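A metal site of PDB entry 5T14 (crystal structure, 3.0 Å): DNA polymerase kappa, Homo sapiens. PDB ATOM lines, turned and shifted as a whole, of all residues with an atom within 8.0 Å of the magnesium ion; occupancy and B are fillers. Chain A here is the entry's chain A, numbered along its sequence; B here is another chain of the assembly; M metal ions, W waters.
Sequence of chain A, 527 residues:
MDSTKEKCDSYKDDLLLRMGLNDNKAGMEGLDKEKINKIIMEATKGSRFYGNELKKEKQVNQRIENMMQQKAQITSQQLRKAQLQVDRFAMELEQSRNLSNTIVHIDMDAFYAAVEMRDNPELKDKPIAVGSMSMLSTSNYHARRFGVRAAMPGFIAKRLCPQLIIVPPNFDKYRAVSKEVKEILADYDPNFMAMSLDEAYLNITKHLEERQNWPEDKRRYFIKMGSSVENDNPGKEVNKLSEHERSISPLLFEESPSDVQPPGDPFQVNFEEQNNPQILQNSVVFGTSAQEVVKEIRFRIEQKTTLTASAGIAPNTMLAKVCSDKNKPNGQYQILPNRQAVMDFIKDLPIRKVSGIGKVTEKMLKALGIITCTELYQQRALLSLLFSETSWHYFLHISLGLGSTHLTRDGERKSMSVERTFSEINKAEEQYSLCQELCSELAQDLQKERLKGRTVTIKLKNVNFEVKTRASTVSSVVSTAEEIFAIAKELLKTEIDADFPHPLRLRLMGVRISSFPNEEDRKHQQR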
ATOM      1  N   LYS A 321       5.850  -6.938  16.911  1.00  0.00           N
ATOM      2  CA  LYS A 321       6.168  -7.499  15.592  1.00  0.00           C
ATOM      3  C   LYS A 321       6.579  -6.442  14.580  1.00  0.00           C
ATOM      4  O   LYS A 321       7.447  -6.698  13.759  1.00  0.00           O
ATOM      5  CB  LYS A 321       4.945  -8.239  15.055  1.00  0.00           C
ATOM      6  CG  LYS A 321       5.112  -8.980  13.729  1.00  0.00           C
ATOM      7  CD  LYS A 321       6.017 -10.178  13.858  1.00  0.00           C
ATOM      8  CE  LYS A 321       5.557 -11.348  12.993  1.00  0.00           C
ATOM      9  NZ  LYS A 321       5.703 -11.054  11.546  1.00  0.00           N
ATOM     10  N   VAL A 322       5.958  -5.266  14.641  1.00  0.00           N
ATOM     11  CA  VAL A 322       6.260  -4.190  13.696  1.00  0.00           C
ATOM     12  C   VAL A 322       7.570  -3.477  14.022  1.00  0.00           C
ATOM     13  O   VAL A 322       8.358  -3.195  13.116  1.00  0.00           O
ATOM     14  CB  VAL A 322       5.111  -3.171  13.600  1.00  0.00           C
ATOM     15  CG1 VAL A 322       5.469  -2.069  12.610  1.00  0.00           C
ATOM     16  CG2 VAL A 322       3.829  -3.854  13.165  1.00  0.00           C
ATOM     17  N   PRO A 350       2.468   2.517   7.688  1.00  0.00           N
ATOM     18  CA  PRO A 350       1.734   1.824   6.610  1.00  0.00           C
ATOM     19  C   PRO A 350       1.107   0.514   7.091  1.00  0.00           C
ATOM     20  O   PRO A 350       1.779  -0.277   7.754  1.00  0.00           O
ATOM     21  CB  PRO A 350       2.818   1.557   5.568  1.00  0.00           C
ATOM     22  CG  PRO A 350       3.921   2.495   5.888  1.00  0.00           C
ATOM     23  CD  PRO A 350       3.889   2.680   7.369  1.00  0.00           C
ATOM     24  N   ILE A 351      -0.164   0.291   6.741  1.00  0.00           N
ATOM     25  CA  ILE A 351      -0.895  -0.893   7.227  1.00  0.00           C
ATOM     26  C   ILE A 351      -0.320  -2.238   6.762  1.00  0.00           C
ATOM     27  O   ILE A 351      -0.473  -3.240   7.460  1.00  0.00           O
ATOM     28  CB  ILE A 351      -2.451  -0.841   6.987  1.00  0.00           C
ATOM     29  CG1 ILE A 351      -2.873  -1.168   5.537  1.00  0.00           C
ATOM     30  CG2 ILE A 351      -3.046   0.472   7.486  1.00  0.00           C
ATOM     31  CD1 ILE A 351      -2.444  -0.190   4.462  1.00  0.00           C
ATOM     32  N   ARG A 352       0.361  -2.261   5.608  1.00  0.00           N
ATOM     33  CA  ARG A 352       1.040  -3.475   5.097  1.00  0.00           C
ATOM     34  C   ARG A 352       2.016  -4.134   6.101  1.00  0.00           C
ATOM     35  O   ARG A 352       2.097  -5.376   6.198  1.00  0.00           O
ATOM     36  CB  ARG A 352       1.803  -3.109   3.831  1.00  0.00           C
ATOM     37  CG  ARG A 352       2.426  -4.283   3.096  1.00  0.00           C
ATOM     38  CD  ARG A 352       1.377  -5.274   2.607  1.00  0.00           C
ATOM     39  NE  ARG A 352       1.848  -6.014   1.432  1.00  0.00           N
ATOM     40  CZ  ARG A 352       2.673  -7.062   1.465  1.00  0.00           C
ATOM     41  NH1 ARG A 352       3.028  -7.645   0.320  1.00  0.00           N
ATOM     42  NH2 ARG A 352       3.124  -7.550   2.621  1.00  0.00           N
ATOM     43  N   LYS A 353       2.733  -3.276   6.820  1.00  0.00           N
ATOM     44  CA  LYS A 353       3.747  -3.696   7.793  1.00  0.00           C
ATOM     45  C   LYS A 353       3.156  -4.388   9.037  1.00  0.00           C
ATOM     46  O   LYS A 353       3.882  -5.052   9.778  1.00  0.00           O
ATOM     47  CB  LYS A 353       4.617  -2.511   8.211  1.00  0.00           C
ATOM     48  CG  LYS A 353       5.354  -1.865   7.043  1.00  0.00           C
ATOM     49  CD  LYS A 353       6.788  -1.483   7.357  1.00  0.00           C
ATOM     50  CE  LYS A 353       6.946  -0.145   8.057  1.00  0.00           C
ATOM     51  NZ  LYS A 353       8.391   0.237   8.173  1.00  0.00           N
ATOM     52  N   VAL A 354       1.855  -4.216   9.258  1.00  0.00           N
ATOM     53  CA  VAL A 354       1.154  -5.013  10.268  1.00  0.00           C
ATOM     54  C   VAL A 354       1.009  -6.463   9.777  1.00  0.00           C
ATOM     55  O   VAL A 354       0.666  -6.725   8.612  1.00  0.00           O
ATOM     56  CB  VAL A 354      -0.232  -4.455  10.605  1.00  0.00           C
ATOM     57  CG1 VAL A 354      -0.880  -5.284  11.687  1.00  0.00           C
ATOM     58  CG2 VAL A 354      -0.127  -3.009  11.084  1.00  0.00           C
ATOM     59  N   SER A 355       1.295  -7.387  10.692  1.00  0.00           N
ATOM     60  CA  SER A 355       1.210  -8.810  10.428  1.00  0.00           C
ATOM     61  C   SER A 355      -0.263  -9.157  10.292  1.00  0.00           C
ATOM     62  O   SER A 355      -1.052  -8.856  11.193  1.00  0.00           O
ATOM     63  CB  SER A 355       1.843  -9.590  11.586  1.00  0.00           C
ATOM     64  OG  SER A 355       1.654 -10.986  11.436  1.00  0.00           O
ATOM     65  N   GLY A 356      -0.641  -9.769   9.171  1.00  0.00           N
ATOM     66  CA  GLY A 356      -2.029 -10.111   8.905  1.00  0.00           C
ATOM     67  C   GLY A 356      -2.691  -9.256   7.839  1.00  0.00           C
ATOM     68  O   GLY A 356      -3.629  -9.716   7.196  1.00  0.00           O
ATOM     69  N   ILE A 357      -2.233  -8.017   7.659  1.00  0.00           N
ATOM     70  CA  ILE A 357      -2.568  -7.224   6.476  1.00  0.00           C
ATOM     71  C   ILE A 357      -1.528  -7.554   5.424  1.00  0.00           C
ATOM     72  O   ILE A 357      -0.348  -7.263   5.600  1.00  0.00           O
ATOM     73  CB  ILE A 357      -2.523  -5.698   6.740  1.00  0.00           C
ATOM     74  CG1 ILE A 357      -3.335  -5.267   7.973  1.00  0.00           C
ATOM     75  CG2 ILE A 357      -3.002  -4.944   5.508  1.00  0.00           C
ATOM     76  CD1 ILE A 357      -4.827  -5.466   7.863  1.00  0.00           C
ATOM     77  N   GLY A 358      -1.941  -8.144   4.322  1.00  0.00           N
ATOM     78  CA  GLY A 358      -1.018  -8.514   3.261  1.00  0.00           C
ATOM     79  C   GLY A 358      -1.292  -7.795   1.965  1.00  0.00           C
ATOM     80  O   GLY A 358      -1.954  -6.763   1.958  1.00  0.00           O
ATOM     81  N   LYS A 359      -0.774  -8.371   0.886  1.00  0.00           N
ATOM     82  CA  LYS A 359      -0.802  -7.776  -0.440  1.00  0.00           C
ATOM     83  C   LYS A 359      -2.201  -7.330  -0.839  1.00  0.00           C
ATOM     84  O   LYS A 359      -2.397  -6.167  -1.196  1.00  0.00           O
ATOM     85  CB  LYS A 359      -0.270  -8.783  -1.458  1.00  0.00           C
ATOM     86  CG  LYS A 359      -0.180  -8.304  -2.903  1.00  0.00           C
ATOM     87  CD  LYS A 359      -0.222  -9.484  -3.856  1.00  0.00           C
ATOM     88  CE  LYS A 359      -0.194  -9.055  -5.313  1.00  0.00           C
ATOM     89  NZ  LYS A 359       1.144  -8.565  -5.753  1.00  0.00           N
ATOM     90  N   GLU A 362      -4.084  -4.648   1.416  1.00  0.00           N
ATOM     91  CA  GLU A 362      -3.419  -3.371   1.128  1.00  0.00           C
ATOM     92  C   GLU A 362      -4.044  -2.713  -0.098  1.00  0.00           C
ATOM     93  O   GLU A 362      -4.495  -1.589  -0.028  1.00  0.00           O
ATOM     94  CB  GLU A 362      -1.911  -3.559   0.931  1.00  0.00           C
ATOM     95  CG  GLU A 362      -1.107  -2.246   0.954  1.00  0.00           C
ATOM     96  CD  GLU A 362       0.348  -2.399   0.521  1.00  0.00           C
ATOM     97  OE1 GLU A 362       1.142  -1.485   0.828  1.00  0.00           O
ATOM     98  OE2 GLU A 362       0.713  -3.412  -0.130  1.00  0.00           O
ATOM     99  N   TYR A 394     -10.917  -6.276  13.711  1.00  0.00           N
ATOM    100  CA  TYR A 394      -9.472  -6.346  13.551  1.00  0.00           C
ATOM    101  C   TYR A 394      -8.918  -4.956  13.192  1.00  0.00           C
ATOM    102  O   TYR A 394      -8.072  -4.435  13.910  1.00  0.00           O
ATOM    103  CB  TYR A 394      -9.124  -7.409  12.492  1.00  0.00           C
ATOM    104  CG  TYR A 394      -7.649  -7.543  12.105  1.00  0.00           C
ATOM    105  CD1 TYR A 394      -6.664  -7.719  13.077  1.00  0.00           C
ATOM    106  CD2 TYR A 394      -7.257  -7.520  10.759  1.00  0.00           C
ATOM    107  CE1 TYR A 394      -5.319  -7.835  12.722  1.00  0.00           C
ATOM    108  CE2 TYR A 394      -5.924  -7.648  10.403  1.00  0.00           C
ATOM    109  CZ  TYR A 394      -4.958  -7.802  11.378  1.00  0.00           C
ATOM    110  OH  TYR A 394      -3.652  -7.932  11.006  1.00  0.00           O
ATOM    111  P    DG B   7      -3.864 -10.659   2.042  1.00  0.00           P
ATOM    112  OP1  DG B   7      -4.282  -9.230   2.105  1.00  0.00           O
ATOM    113  OP2  DG B   7      -3.041 -11.129   0.895  1.00  0.00           O
ATOM    114  O5'  DG B   7      -3.086 -10.994   3.386  1.00  0.00           O
ATOM    115  C5'  DG B   7      -3.660 -11.758   4.457  1.00  0.00           C
ATOM    116  C4'  DG B   7      -2.595 -12.481   5.254  1.00  0.00           C
ATOM    117  O4'  DG B   7      -2.730 -13.889   4.986  1.00  0.00           O
ATOM    118  C3'  DG B   7      -1.135 -12.105   4.967  1.00  0.00           C
ATOM    119  O3'  DG B   7      -0.505 -11.537   6.120  1.00  0.00           O
ATOM    120  C2'  DG B   7      -0.495 -13.401   4.476  1.00  0.00           C
ATOM    121  C1'  DG B   7      -1.452 -14.490   4.923  1.00  0.00           C
ATOM    122  N9   DG B   7      -1.550 -15.641   4.020  1.00  0.00           N
ATOM    123  C8   DG B   7      -1.668 -15.632   2.648  1.00  0.00           C
ATOM    124  N7   DG B   7      -1.745 -16.828   2.138  1.00  0.00           N
ATOM    125  C5   DG B   7      -1.686 -17.671   3.234  1.00  0.00           C
ATOM    126  C6   DG B   7      -1.712 -19.090   3.297  1.00  0.00           C
ATOM    127  O6   DG B   7      -1.801 -19.906   2.378  1.00  0.00           O
ATOM    128  N1   DG B   7      -1.623 -19.549   4.608  1.00  0.00           N
ATOM    129  C2   DG B   7      -1.516 -18.744   5.722  1.00  0.00           C
ATOM    130  N2   DG B   7      -1.438 -19.361   6.908  1.00  0.00           N
ATOM    131  N3   DG B   7      -1.493 -17.413   5.669  1.00  0.00           N
ATOM    132  C4   DG B   7      -1.580 -16.959   4.407  1.00  0.00           C
ATOM    133  P    DA B   8       0.995 -10.951   6.027  1.00  0.00           P
ATOM    134  OP1  DA B   8       1.043  -9.603   6.674  1.00  0.00           O
ATOM    135  OP2  DA B   8       1.472 -11.119   4.629  1.00  0.00           O
ATOM    136  O5'  DA B   8       1.827 -11.990   6.912  1.00  0.00           O
ATOM    137  C5'  DA B   8       1.361 -12.490   8.181  1.00  0.00           C
ATOM    138  C4'  DA B   8       2.106 -13.773   8.495  1.00  0.00           C
ATOM    139  O4'  DA B   8       1.554 -14.844   7.702  1.00  0.00           O
ATOM    140  C3'  DA B   8       3.603 -13.718   8.141  1.00  0.00           C
ATOM    141  O3'  DA B   8       4.496 -13.683   9.251  1.00  0.00           O
ATOM    142  C2'  DA B   8       3.834 -14.974   7.315  1.00  0.00           C
ATOM    143  C1'  DA B   8       2.566 -15.782   7.466  1.00  0.00           C
ATOM    144  N9   DA B   8       2.270 -16.485   6.221  1.00  0.00           N
ATOM    145  C8   DA B   8       2.204 -15.923   4.971  1.00  0.00           C
ATOM    146  N7   DA B   8       2.008 -16.795   4.012  1.00  0.00           N
ATOM    147  C5   DA B   8       1.972 -18.009   4.674  1.00  0.00           C
ATOM    148  C6   DA B   8       1.790 -19.327   4.216  1.00  0.00           C
ATOM    149  N6   DA B   8       1.596 -19.642   2.921  1.00  0.00           N
ATOM    150  N1   DA B   8       1.809 -20.317   5.128  1.00  0.00           N
ATOM    151  C2   DA B   8       1.984 -19.998   6.416  1.00  0.00           C
ATOM    152  N3   DA B   8       2.175 -18.806   6.971  1.00  0.00           N
ATOM    153  C4   DA B   8       2.151 -17.844   6.027  1.00  0.00           C
ATOM    154  P    DC B   9       6.079 -13.523   8.993  1.00  0.00           P
ATOM    155  OP1  DC B   9       6.695 -13.007  10.235  1.00  0.00           O
ATOM    156  OP2  DC B   9       6.270 -12.813   7.685  1.00  0.00           O
ATOM    157  O5'  DC B   9       6.564 -15.022   8.772  1.00  0.00           O
ATOM    158  C5'  DC B   9       6.126 -16.091   9.648  1.00  0.00           C
ATOM    159  C4'  DC B   9       7.008 -17.303   9.464  1.00  0.00           C
ATOM    160  O4'  DC B   9       6.541 -18.071   8.332  1.00  0.00           O
ATOM    161  C3'  DC B   9       8.478 -16.994   9.193  1.00  0.00           C
ATOM    162  O3'  DC B   9       9.333 -17.951   9.819  1.00  0.00           O
ATOM    163  C2'  DC B   9       8.589 -17.119   7.688  1.00  0.00           C
ATOM    164  C1'  DC B   9       7.582 -18.200   7.372  1.00  0.00           C
ATOM    165  N1   DC B   9       6.959 -18.127   6.036  1.00  0.00           N
ATOM    166  C2   DC B   9       6.763 -19.308   5.305  1.00  0.00           C
ATOM    167  O2   DC B   9       7.172 -20.376   5.793  1.00  0.00           O
ATOM    168  N3   DC B   9       6.188 -19.248   4.089  1.00  0.00           N
ATOM    169  C4   DC B   9       5.783 -18.074   3.601  1.00  0.00           C
ATOM    170  N4   DC B   9       5.217 -18.054   2.392  1.00  0.00           N
ATOM    171  C5   DC B   9       5.960 -16.851   4.320  1.00  0.00           C
ATOM    172  C6   DC B   9       6.535 -16.929   5.526  1.00  0.00           C
HETATM  173 MG    MG M   1       1.523  -7.453   6.719  1.00  0.00          MG
HETATM  174  O   HOH W   1       3.596  -7.828   7.265  1.00  0.00           O
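O of Ser 355 is in hydrogen-bond range of OH of Tyr 394. OP1 of DA 8 of chain B lies close to the backbone NH (N) of Gly 356 (3.0 Å). The guanidinium group (NE) of Arg 352 is in salt-bridge range of the side-chain carboxylate (OE2) of Glu 362 (3.2 Å).
Ser 355 touches the magnesium ion.
The magnesium ion is bound by water W1 (2.2 Å), O of Ile 357 (2.2 Å), O of Val 354 (2.2 Å), OP1 of DA 8 of chain B (2.2 Å) and O of Arg 352 (2.2 Å).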
